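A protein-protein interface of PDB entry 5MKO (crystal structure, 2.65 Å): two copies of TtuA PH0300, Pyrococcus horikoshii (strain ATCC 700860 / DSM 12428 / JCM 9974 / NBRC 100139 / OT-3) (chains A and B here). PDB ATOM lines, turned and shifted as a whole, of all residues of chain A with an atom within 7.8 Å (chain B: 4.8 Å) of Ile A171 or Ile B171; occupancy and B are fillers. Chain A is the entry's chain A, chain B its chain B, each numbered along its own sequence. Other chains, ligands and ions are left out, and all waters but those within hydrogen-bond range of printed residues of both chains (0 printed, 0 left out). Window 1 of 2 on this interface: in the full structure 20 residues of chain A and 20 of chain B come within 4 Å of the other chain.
The indole nitrogen of Trp A174 lies within hydrogen-bond range of the backbone carbonyl oxygen of Phe B252 (2.8 Å). O of Phe A252 sits at hydrogen-bond distance from NE1 of Trp B174 (2.8 Å). The backbone NH (N) of Tyr A256 sits close to the indole nitrogen (NE1) of Trp B174 (3.3 Å).
The indole nitrogen (NE1) of Trp A174 lies within hydrogen-bond range of the backbone carbonyl oxygen (O) of Ile A171. The side-chain hydroxyl (OH) of Tyr A256 sits at hydrogen-bond distance from the backbone carbonyl oxygen (O) of Leu A179, 2.7 Å away. NE1 of Trp B174 sits at hydrogen-bond distance from O of Ile B171.
Among the printed residues, merely in contact across the chains: Gly A255 with Trp B174, Phe A252 with Leu B172, Leu A172 with Phe B252, Ile A171 with Ile B171, Phe A252 with Ile B171, Ile A171 with Phe B252, Phe A263 with Trp B174, Trp A174 with Phe B263, Leu A168 with Leu B168, Trp A174 with Ile B171 and Ile A171 with Trp B174.
Ile A171 touches three residues of chain B. Ile B171 touches just these residues of chain A: Ile A171, Trp A174 and Phe A252. Of the printed residues of chain B, Leu A172 touches Phe B252. Of the printed residues of chain A, Leu B168 touches Leu A168 (3.8 Å).
Hydrophobic or aromatic side chains of chain A that line the printed part of chain B: Leu A168, Ile A171, Leu A172, Trp A174, Phe A252, Tyr A256 and Phe A263. Of the 11 printed residues of chain B, 6 touch a printed residue of chain A. Printed residues of chain B that touch a printed residue of chain A: Leu B168, Ile B171, Leu B172, Trp B174, Phe B252 and Phe B263. Among the printed residues, 14 pairs touch across the chains. Among the printed residues, no Asp or Glu carboxylate lies within 4 Å of a Lys or Arg side-chain nitrogen of the other chain.
Ile A171 touches its own counterpart, Ile B171. Ile A171 touches Phe B252, and with the chains exchanged Phe A252 touches Ile B171. Trp A174 touches Phe B252, and with the chains exchanged Phe A252 touches Trp B174. Trp A174 touches Phe B263, and with the chains exchanged Phe A263 touches Trp B174. Positions printed for both chains: 167, 168, 169, 170, 171, 172, 173, 174, 179, 252 and 263. Of the 14 pairs that touch across the chains among the printed residues, 12 have their exchanged pair printed and touching as well.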
ATOM      1  N   GLU A 163     -21.318  -4.835  14.507  1.00  0.00           N
ATOM      2  CA  GLU A 163     -21.851  -5.304  15.781  1.00  0.00           C
ATOM      3  C   GLU A 163     -21.074  -4.725  16.967  1.00  0.00           C
ATOM      4  O   GLU A 163     -21.694  -4.220  17.916  1.00  0.00           O
ATOM      5  CB  GLU A 163     -21.889  -6.839  15.811  1.00  0.00           C
ATOM      6  CG  GLU A 163     -22.755  -7.386  16.927  1.00  0.00           C
ATOM      7  CD  GLU A 163     -24.276  -7.284  16.868  1.00  0.00           C
ATOM      8  OE1 GLU A 163     -24.847  -6.602  15.982  1.00  0.00           O
ATOM      9  OE2 GLU A 163     -24.907  -7.963  17.710  1.00  0.00           O
ATOM     10  N   ALA A 164     -19.720  -4.772  16.900  1.00  0.00           N
ATOM     11  CA  ALA A 164     -18.833  -4.235  17.935  1.00  0.00           C
ATOM     12  C   ALA A 164     -19.130  -2.751  18.176  1.00  0.00           C
ATOM     13  O   ALA A 164     -19.358  -2.373  19.323  1.00  0.00           O
ATOM     14  CB  ALA A 164     -17.373  -4.445  17.549  1.00  0.00           C
ATOM     15  N   SER A 165     -19.220  -1.939  17.095  1.00  0.00           N
ATOM     16  CA  SER A 165     -19.531  -0.502  17.163  1.00  0.00           C
ATOM     17  C   SER A 165     -20.949  -0.203  17.676  1.00  0.00           C
ATOM     18  O   SER A 165     -21.131   0.763  18.413  1.00  0.00           O
ATOM     19  CB  SER A 165     -19.265   0.188  15.828  1.00  0.00           C
ATOM     20  OG  SER A 165     -20.025  -0.400  14.787  1.00  0.00           O
ATOM     21  N   PHE A 166     -21.934  -1.037  17.319  1.00  0.00           N
ATOM     22  CA  PHE A 166     -23.314  -0.887  17.790  1.00  0.00           C
ATOM     23  C   PHE A 166     -23.358  -1.147  19.306  1.00  0.00           C
ATOM     24  O   PHE A 166     -24.032  -0.412  20.031  1.00  0.00           O
ATOM     25  CB  PHE A 166     -24.268  -1.831  17.022  1.00  0.00           C
ATOM     26  CG  PHE A 166     -25.658  -1.981  17.607  1.00  0.00           C
ATOM     27  CD1 PHE A 166     -26.686  -1.114  17.236  1.00  0.00           C
ATOM     28  CD2 PHE A 166     -25.948  -3.006  18.512  1.00  0.00           C
ATOM     29  CE1 PHE A 166     -27.974  -1.249  17.783  1.00  0.00           C
ATOM     30  CE2 PHE A 166     -27.228  -3.133  19.071  1.00  0.00           C
ATOM     31  CZ  PHE A 166     -28.233  -2.252  18.704  1.00  0.00           C
ATOM     32  N   LEU A 167     -22.628  -2.190  19.777  1.00  0.00           N
ATOM     33  CA  LEU A 167     -22.537  -2.529  21.195  1.00  0.00           C
ATOM     34  C   LEU A 167     -21.882  -1.396  21.950  1.00  0.00           C
ATOM     35  O   LEU A 167     -22.464  -0.899  22.912  1.00  0.00           O
ATOM     36  CB  LEU A 167     -21.715  -3.804  21.420  1.00  0.00           C
ATOM     37  CG  LEU A 167     -22.327  -5.138  21.073  1.00  0.00           C
ATOM     38  CD1 LEU A 167     -21.370  -6.259  21.447  1.00  0.00           C
ATOM     39  CD2 LEU A 167     -23.683  -5.318  21.737  1.00  0.00           C
ATOM     40  N   LEU A 168     -20.691  -0.958  21.486  1.00  0.00           N
ATOM     41  CA  LEU A 168     -19.951   0.145  22.084  1.00  0.00           C
ATOM     42  C   LEU A 168     -20.789   1.413  22.169  1.00  0.00           C
ATOM     43  O   LEU A 168     -20.814   2.043  23.217  1.00  0.00           O
ATOM     44  CB  LEU A 168     -18.635   0.406  21.325  1.00  0.00           C
ATOM     45  CG  LEU A 168     -17.670   1.409  21.975  1.00  0.00           C
ATOM     46  CD1 LEU A 168     -17.171   0.915  23.323  1.00  0.00           C
ATOM     47  CD2 LEU A 168     -16.514   1.718  21.073  1.00  0.00           C
ATOM     48  N   ASN A 169     -21.492   1.770  21.099  1.00  0.00           N
ATOM     49  CA  ASN A 169     -22.311   2.972  21.099  1.00  0.00           C
ATOM     50  C   ASN A 169     -23.480   2.905  22.083  1.00  0.00           C
ATOM     51  O   ASN A 169     -23.759   3.897  22.758  1.00  0.00           O
ATOM     52  CB  ASN A 169     -22.779   3.330  19.690  1.00  0.00           C
ATOM     53  CG  ASN A 169     -23.439   4.678  19.606  1.00  0.00           C
ATOM     54  OD1 ASN A 169     -22.973   5.673  20.184  1.00  0.00           O
ATOM     55  ND2 ASN A 169     -24.557   4.735  18.903  1.00  0.00           N
ATOM     56  N   ASN A 170     -24.143   1.740  22.189  1.00  0.00           N
ATOM     57  CA  ASN A 170     -25.284   1.584  23.095  1.00  0.00           C
ATOM     58  C   ASN A 170     -24.872   1.322  24.521  1.00  0.00           C
ATOM     59  O   ASN A 170     -25.675   1.549  25.427  1.00  0.00           O
ATOM     60  CB  ASN A 170     -26.272   0.547  22.594  1.00  0.00           C
ATOM     61  CG  ASN A 170     -26.937   0.972  21.314  1.00  0.00           C
ATOM     62  OD1 ASN A 170     -27.586   2.025  21.219  1.00  0.00           O
ATOM     63  ND2 ASN A 170     -26.735   0.191  20.292  1.00  0.00           N
ATOM     64  N   ILE A 171     -23.619   0.888  24.735  1.00  0.00           N
ATOM     65  CA  ILE A 171     -23.075   0.688  26.080  1.00  0.00           C
ATOM     66  C   ILE A 171     -22.757   2.066  26.641  1.00  0.00           C
ATOM     67  O   ILE A 171     -23.132   2.353  27.771  1.00  0.00           O
ATOM     68  CB  ILE A 171     -21.889  -0.308  26.102  1.00  0.00           C
ATOM     69  CG1 ILE A 171     -22.415  -1.755  26.152  1.00  0.00           C
ATOM     70  CG2 ILE A 171     -20.918  -0.032  27.242  1.00  0.00           C
ATOM     71  CD1 ILE A 171     -21.676  -2.672  25.398  1.00  0.00           C
ATOM     72  N   LEU A 172     -22.150   2.940  25.814  1.00  0.00           N
ATOM     73  CA  LEU A 172     -21.813   4.323  26.164  1.00  0.00           C
ATOM     74  C   LEU A 172     -23.047   5.166  26.498  1.00  0.00           C
ATOM     75  O   LEU A 172     -22.975   6.015  27.384  1.00  0.00           O
ATOM     76  CB  LEU A 172     -21.017   4.987  25.033  1.00  0.00           C
ATOM     77  CG  LEU A 172     -19.545   4.598  24.889  1.00  0.00           C
ATOM     78  CD1 LEU A 172     -19.001   5.088  23.566  1.00  0.00           C
ATOM     79  CD2 LEU A 172     -18.698   5.142  26.039  1.00  0.00           C
ATOM     80  N   HIS A 173     -24.172   4.926  25.792  1.00  0.00           N
ATOM     81  CA  HIS A 173     -25.445   5.615  25.995  1.00  0.00           C
ATOM     82  C   HIS A 173     -26.375   4.870  26.940  1.00  0.00           C
ATOM     83  O   HIS A 173     -27.422   5.407  27.313  1.00  0.00           O
ATOM     84  CB  HIS A 173     -26.147   5.841  24.656  1.00  0.00           C
ATOM     85  CG  HIS A 173     -25.496   6.891  23.830  1.00  0.00           C
ATOM     86  ND1 HIS A 173     -24.869   6.585  22.641  1.00  0.00           N
ATOM     87  CD2 HIS A 173     -25.366   8.216  24.067  1.00  0.00           C
ATOM     88  CE1 HIS A 173     -24.389   7.728  22.185  1.00  0.00           C
ATOM     89  NE2 HIS A 173     -24.652   8.736  23.017  1.00  0.00           N
ATOM     90  N   TRP A 174     -26.001   3.630  27.320  1.00  0.00           N
ATOM     91  CA  TRP A 174     -26.769   2.733  28.189  1.00  0.00           C
ATOM     92  C   TRP A 174     -28.214   2.549  27.666  1.00  0.00           C
ATOM     93  O   TRP A 174     -29.194   2.732  28.398  1.00  0.00           O
ATOM     94  CB  TRP A 174     -26.675   3.135  29.672  1.00  0.00           C
ATOM     95  CG  TRP A 174     -25.308   2.853  30.228  1.00  0.00           C
ATOM     96  CD1 TRP A 174     -24.273   3.734  30.350  1.00  0.00           C
ATOM     97  CD2 TRP A 174     -24.786   1.569  30.598  1.00  0.00           C
ATOM     98  NE1 TRP A 174     -23.149   3.086  30.808  1.00  0.00           N
ATOM     99  CE2 TRP A 174     -23.437   1.756  30.975  1.00  0.00           C
ATOM    100  CE3 TRP A 174     -25.337   0.279  30.681  1.00  0.00           C
ATOM    101  CZ2 TRP A 174     -22.632   0.702  31.426  1.00  0.00           C
ATOM    102  CZ3 TRP A 174     -24.537  -0.764  31.127  1.00  0.00           C
ATOM    103  CH2 TRP A 174     -23.202  -0.548  31.492  1.00  0.00           C
ATOM    104  N   ASN A 175     -28.299   2.196  26.355  1.00  0.00           N
ATOM    105  CA  ASN A 175     -29.510   1.883  25.604  1.00  0.00           C
ATOM    106  C   ASN A 175     -29.712   0.384  25.774  1.00  0.00           C
ATOM    107  O   ASN A 175     -29.410  -0.411  24.877  1.00  0.00           O
ATOM    108  CB  ASN A 175     -29.360   2.247  24.116  1.00  0.00           C
ATOM    109  CG  ASN A 175     -29.397   3.722  23.799  1.00  0.00           C
ATOM    110  OD1 ASN A 175     -30.165   4.496  24.383  1.00  0.00           O
ATOM    111  ND2 ASN A 175     -28.602   4.133  22.816  1.00  0.00           N
ATOM    112  N   THR A 176     -30.187   0.010  26.967  1.00  0.00           N
ATOM    113  CA  THR A 176     -30.410  -1.360  27.422  1.00  0.00           C
ATOM    114  C   THR A 176     -31.503  -2.098  26.645  1.00  0.00           C
ATOM    115  O   THR A 176     -31.497  -3.331  26.628  1.00  0.00           O
ATOM    116  CB  THR A 176     -30.661  -1.369  28.926  1.00  0.00           C
ATOM    117  OG1 THR A 176     -31.729  -0.464  29.222  1.00  0.00           O
ATOM    118  CG2 THR A 176     -29.414  -0.999  29.725  1.00  0.00           C
ATOM    119  N   LEU A 179     -29.680  -3.158  23.489  1.00  0.00           N
ATOM    120  CA  LEU A 179     -28.713  -4.165  23.924  1.00  0.00           C
ATOM    121  C   LEU A 179     -29.347  -5.530  24.129  1.00  0.00           C
ATOM    122  O   LEU A 179     -28.647  -6.535  24.091  1.00  0.00           O
ATOM    123  CB  LEU A 179     -27.965  -3.712  25.190  1.00  0.00           C
ATOM    124  CG  LEU A 179     -26.899  -2.635  24.985  1.00  0.00           C
ATOM    125  CD1 LEU A 179     -26.398  -2.106  26.315  1.00  0.00           C
ATOM    126  CD2 LEU A 179     -25.746  -3.139  24.120  1.00  0.00           C
ATOM    127  N   ASN A 251     -14.130 -11.194  21.273  1.00  0.00           N
ATOM    128  CA  ASN A 251     -14.440 -11.490  22.670  1.00  0.00           C
ATOM    129  C   ASN A 251     -15.469 -10.547  23.274  1.00  0.00           C
ATOM    130  O   ASN A 251     -16.217 -10.964  24.152  1.00  0.00           O
ATOM    131  CB  ASN A 251     -13.165 -11.542  23.503  1.00  0.00           C
ATOM    132  CG  ASN A 251     -12.150 -12.538  23.001  1.00  0.00           C
ATOM    133  OD1 ASN A 251     -12.474 -13.532  22.350  1.00  0.00           O
ATOM    134  ND2 ASN A 251     -10.887 -12.269  23.258  1.00  0.00           N
ATOM    135  N   PHE A 252     -15.519  -9.292  22.799  1.00  0.00           N
ATOM    136  CA  PHE A 252     -16.497  -8.293  23.226  1.00  0.00           C
ATOM    137  C   PHE A 252     -17.891  -8.710  22.753  1.00  0.00           C
ATOM    138  O   PHE A 252     -18.844  -8.668  23.527  1.00  0.00           O
ATOM    139  CB  PHE A 252     -16.127  -6.907  22.661  1.00  0.00           C
ATOM    140  CG  PHE A 252     -17.086  -5.777  22.968  1.00  0.00           C
ATOM    141  CD1 PHE A 252     -17.669  -5.656  24.230  1.00  0.00           C
ATOM    142  CD2 PHE A 252     -17.361  -4.802  22.017  1.00  0.00           C
ATOM    143  CE1 PHE A 252     -18.565  -4.621  24.508  1.00  0.00           C
ATOM    144  CE2 PHE A 252     -18.232  -3.749  22.307  1.00  0.00           C
ATOM    145  CZ  PHE A 252     -18.821  -3.661  23.553  1.00  0.00           C
ATOM    146  N   VAL A 253     -17.996  -9.129  21.488  1.00  0.00           N
ATOM    147  CA  VAL A 253     -19.254  -9.538  20.877  1.00  0.00           C
ATOM    148  C   VAL A 253     -19.718 -10.910  21.421  1.00  0.00           C
ATOM    149  O   VAL A 253     -20.885 -11.043  21.806  1.00  0.00           O
ATOM    150  CB  VAL A 253     -19.159  -9.456  19.335  1.00  0.00           C
ATOM    151  CG1 VAL A 253     -20.351 -10.129  18.663  1.00  0.00           C
ATOM    152  CG2 VAL A 253     -19.043  -7.997  18.885  1.00  0.00           C
ATOM    153  N   GLY A 255     -18.739 -12.345  24.247  1.00  0.00           N
ATOM    154  CA  GLY A 255     -18.968 -12.146  25.673  1.00  0.00           C
ATOM    155  C   GLY A 255     -20.338 -11.554  25.915  1.00  0.00           C
ATOM    156  O   GLY A 255     -21.031 -11.943  26.858  1.00  0.00           O
ATOM    157  N   TYR A 256     -20.746 -10.632  25.027  1.00  0.00           N
ATOM    158  CA  TYR A 256     -22.045  -9.973  25.048  1.00  0.00           C
ATOM    159  C   TYR A 256     -23.179 -10.980  24.852  1.00  0.00           C
ATOM    160  O   TYR A 256     -24.215 -10.838  25.494  1.00  0.00           O
ATOM    161  CB  TYR A 256     -22.097  -8.841  24.002  1.00  0.00           C
ATOM    162  CG  TYR A 256     -23.485  -8.519  23.492  1.00  0.00           C
ATOM    163  CD1 TYR A 256     -24.401  -7.830  24.284  1.00  0.00           C
ATOM    164  CD2 TYR A 256     -23.893  -8.927  22.225  1.00  0.00           C
ATOM    165  CE1 TYR A 256     -25.690  -7.566  23.834  1.00  0.00           C
ATOM    166  CE2 TYR A 256     -25.180  -8.661  21.761  1.00  0.00           C
ATOM    167  CZ  TYR A 256     -26.070  -7.971  22.565  1.00  0.00           C
ATOM    168  OH  TYR A 256     -27.331  -7.700  22.102  1.00  0.00           O
ATOM    169  N   PHE A 263     -29.892  -7.934  29.908  1.00  0.00           N
ATOM    170  CA  PHE A 263     -30.570  -6.773  29.323  1.00  0.00           C
ATOM    171  C   PHE A 263     -32.000  -7.103  28.926  1.00  0.00           C
ATOM    172  O   PHE A 263     -32.791  -6.189  28.705  1.00  0.00           O
ATOM    173  CB  PHE A 263     -29.795  -6.219  28.118  1.00  0.00           C
ATOM    174  CG  PHE A 263     -28.353  -5.869  28.384  1.00  0.00           C
ATOM    175  CD1 PHE A 263     -28.021  -4.740  29.127  1.00  0.00           C
ATOM    176  CD2 PHE A 263     -27.327  -6.651  27.871  1.00  0.00           C
ATOM    177  CE1 PHE A 263     -26.684  -4.415  29.373  1.00  0.00           C
ATOM    178  CE2 PHE A 263     -25.991  -6.318  28.104  1.00  0.00           C
ATOM    179  CZ  PHE A 263     -25.679  -5.201  28.854  1.00  0.00           C
ATOM    180  N   LEU B 167     -14.803   0.688  33.670  1.00  0.00           N
ATOM    181  CA  LEU B 167     -16.073   0.267  33.068  1.00  0.00           C
ATOM    182  C   LEU B 167     -15.823  -0.268  31.674  1.00  0.00           C
ATOM    183  O   LEU B 167     -16.213  -1.393  31.387  1.00  0.00           O
ATOM    184  CB  LEU B 167     -17.070   1.424  32.977  1.00  0.00           C
ATOM    185  CG  LEU B 167     -17.740   1.909  34.234  1.00  0.00           C
ATOM    186  CD1 LEU B 167     -18.728   3.019  33.902  1.00  0.00           C
ATOM    187  CD2 LEU B 167     -18.407   0.770  34.980  1.00  0.00           C
ATOM    188  N   LEU B 168     -15.132   0.520  30.827  1.00  0.00           N
ATOM    189  CA  LEU B 168     -14.792   0.135  29.464  1.00  0.00           C
ATOM    190  C   LEU B 168     -14.031  -1.181  29.417  1.00  0.00           C
ATOM    191  O   LEU B 168     -14.371  -2.036  28.617  1.00  0.00           O
ATOM    192  CB  LEU B 168     -14.000   1.245  28.754  1.00  0.00           C
ATOM    193  CG  LEU B 168     -13.763   1.047  27.254  1.00  0.00           C
ATOM    194  CD1 LEU B 168     -15.076   1.033  26.479  1.00  0.00           C
ATOM    195  CD2 LEU B 168     -12.833   2.097  26.713  1.00  0.00           C
ATOM    196  N   ASN B 169     -13.036  -1.358  30.284  1.00  0.00           N
ATOM    197  CA  ASN B 169     -12.253  -2.584  30.294  1.00  0.00           C
ATOM    198  C   ASN B 169     -13.072  -3.811  30.699  1.00  0.00           C
ATOM    199  O   ASN B 169     -12.906  -4.871  30.095  1.00  0.00           O
ATOM    200  CB  ASN B 169     -10.993  -2.433  31.148  1.00  0.00           C
ATOM    201  CG  ASN B 169     -10.045  -3.598  31.018  1.00  0.00           C
ATOM    202  OD1 ASN B 169      -9.779  -4.104  29.923  1.00  0.00           O
ATOM    203  ND2 ASN B 169      -9.536  -4.068  32.139  1.00  0.00           N
ATOM    204  N   ASN B 170     -13.963  -3.667  31.691  1.00  0.00           N
ATOM    205  CA  ASN B 170     -14.783  -4.789  32.150  1.00  0.00           C
ATOM    206  C   ASN B 170     -15.994  -5.035  31.280  1.00  0.00           C
ATOM    207  O   ASN B 170     -16.547  -6.133  31.321  1.00  0.00           O
ATOM    208  CB  ASN B 170     -15.162  -4.652  33.613  1.00  0.00           C
ATOM    209  CG  ASN B 170     -13.961  -4.743  34.518  1.00  0.00           C
ATOM    210  OD1 ASN B 170     -13.202  -5.726  34.531  1.00  0.00           O
ATOM    211  ND2 ASN B 170     -13.740  -3.689  35.249  1.00  0.00           N
ATOM    212  N   ILE B 171     -16.394  -4.037  30.472  1.00  0.00           N
ATOM    213  CA  ILE B 171     -17.486  -4.194  29.518  1.00  0.00           C
ATOM    214  C   ILE B 171     -16.954  -5.005  28.348  1.00  0.00           C
ATOM    215  O   ILE B 171     -17.610  -5.954  27.931  1.00  0.00           O
ATOM    216  CB  ILE B 171     -18.140  -2.845  29.124  1.00  0.00           C
ATOM    217  CG1 ILE B 171     -19.166  -2.376  30.201  1.00  0.00           C
ATOM    218  CG2 ILE B 171     -18.736  -2.876  27.720  1.00  0.00           C
ATOM    219  CD1 ILE B 171     -20.628  -3.095  30.340  1.00  0.00           C
ATOM    220  N   LEU B 172     -15.730  -4.686  27.890  1.00  0.00           N
ATOM    221  CA  LEU B 172     -15.032  -5.386  26.810  1.00  0.00           C
ATOM    222  C   LEU B 172     -14.760  -6.856  27.144  1.00  0.00           C
ATOM    223  O   LEU B 172     -14.828  -7.700  26.250  1.00  0.00           O
ATOM    224  CB  LEU B 172     -13.716  -4.672  26.465  1.00  0.00           C
ATOM    225  CG  LEU B 172     -13.805  -3.382  25.651  1.00  0.00           C
ATOM    226  CD1 LEU B 172     -12.479  -2.665  25.662  1.00  0.00           C
ATOM    227  CD2 LEU B 172     -14.230  -3.649  24.211  1.00  0.00           C
ATOM    228  N   HIS B 173     -14.458  -7.154  28.421  1.00  0.00           N
ATOM    229  CA  HIS B 173     -14.192  -8.508  28.922  1.00  0.00           C
ATOM    230  C   HIS B 173     -15.428  -9.173  29.503  1.00  0.00           C
ATOM    231  O   HIS B 173     -15.382 -10.361  29.828  1.00  0.00           O
ATOM    232  CB  HIS B 173     -13.084  -8.479  29.976  1.00  0.00           C
ATOM    233  CG  HIS B 173     -11.735  -8.227  29.393  1.00  0.00           C
ATOM    234  ND1 HIS B 173     -11.046  -7.063  29.653  1.00  0.00           N
ATOM    235  CD2 HIS B 173     -11.006  -8.987  28.546  1.00  0.00           C
ATOM    236  CE1 HIS B 173      -9.916  -7.158  28.976  1.00  0.00           C
ATOM    237  NE2 HIS B 173      -9.850  -8.297  28.293  1.00  0.00           N
ATOM    238  N   TRP B 174     -16.531  -8.409  29.639  1.00  0.00           N
ATOM    239  CA  TRP B 174     -17.812  -8.848  30.200  1.00  0.00           C
ATOM    240  C   TRP B 174     -17.620  -9.487  31.592  1.00  0.00           C
ATOM    241  O   TRP B 174     -18.080 -10.609  31.859  1.00  0.00           O
ATOM    242  CB  TRP B 174     -18.620  -9.711  29.212  1.00  0.00           C
ATOM    243  CG  TRP B 174     -19.161  -8.890  28.080  1.00  0.00           C
ATOM    244  CD1 TRP B 174     -18.603  -8.732  26.847  1.00  0.00           C
ATOM    245  CD2 TRP B 174     -20.282  -7.993  28.130  1.00  0.00           C
ATOM    246  NE1 TRP B 174     -19.329  -7.827  26.110  1.00  0.00           N
ATOM    247  CE2 TRP B 174     -20.369  -7.360  26.870  1.00  0.00           C
ATOM    248  CE3 TRP B 174     -21.236  -7.678  29.112  1.00  0.00           C
ATOM    249  CZ2 TRP B 174     -21.382  -6.446  26.558  1.00  0.00           C
ATOM    250  CZ3 TRP B 174     -22.235  -6.770  28.803  1.00  0.00           C
ATOM    251  CH2 TRP B 174     -22.317  -6.183  27.530  1.00  0.00           C
ATOM    252  N   LEU B 179     -18.482  -5.357  37.447  1.00  0.00           N
ATOM    253  CA  LEU B 179     -19.441  -4.340  37.016  1.00  0.00           C
ATOM    254  C   LEU B 179     -20.550  -4.118  38.030  1.00  0.00           C
ATOM    255  O   LEU B 179     -21.176  -3.064  38.020  1.00  0.00           O
ATOM    256  CB  LEU B 179     -20.025  -4.677  35.634  1.00  0.00           C
ATOM    257  CG  LEU B 179     -19.099  -4.450  34.443  1.00  0.00           C
ATOM    258  CD1 LEU B 179     -19.696  -5.030  33.172  1.00  0.00           C
ATOM    259  CD2 LEU B 179     -18.761  -2.977  34.261  1.00  0.00           C
ATOM    260  N   PHE B 252     -21.514   8.043  30.441  1.00  0.00           N
ATOM    261  CA  PHE B 252     -21.194   6.627  30.464  1.00  0.00           C
ATOM    262  C   PHE B 252     -21.196   6.131  31.909  1.00  0.00           C
ATOM    263  O   PHE B 252     -21.781   5.090  32.200  1.00  0.00           O
ATOM    264  CB  PHE B 252     -19.830   6.379  29.797  1.00  0.00           C
ATOM    265  CG  PHE B 252     -19.330   4.955  29.804  1.00  0.00           C
ATOM    266  CD1 PHE B 252     -20.192   3.893  29.544  1.00  0.00           C
ATOM    267  CD2 PHE B 252     -17.985   4.675  30.009  1.00  0.00           C
ATOM    268  CE1 PHE B 252     -19.730   2.582  29.553  1.00  0.00           C
ATOM    269  CE2 PHE B 252     -17.520   3.362  29.996  1.00  0.00           C
ATOM    270  CZ  PHE B 252     -18.396   2.324  29.763  1.00  0.00           C
ATOM    271  N   PHE B 263     -26.441  -5.882  36.745  1.00  0.00           N
ATOM    272  CA  PHE B 263     -25.258  -6.718  36.962  1.00  0.00           C
ATOM    273  C   PHE B 263     -25.257  -7.339  38.352  1.00  0.00           C
ATOM    274  O   PHE B 263     -24.513  -8.292  38.589  1.00  0.00           O
ATOM    275  CB  PHE B 263     -23.961  -5.922  36.732  1.00  0.00           C
ATOM    276  CG  PHE B 263     -23.851  -5.252  35.388  1.00  0.00           C
ATOM    277  CD1 PHE B 263     -23.609  -5.997  34.238  1.00  0.00           C
ATOM    278  CD2 PHE B 263     -23.964  -3.873  35.270  1.00  0.00           C
ATOM    279  CE1 PHE B 263     -23.512  -5.378  32.991  1.00  0.00           C
ATOM    280  CE2 PHE B 263     -23.849  -3.250  34.025  1.00  0.00           C
ATOM    281  CZ  PHE B 263     -23.623  -4.007  32.894  1.00  0.00           C
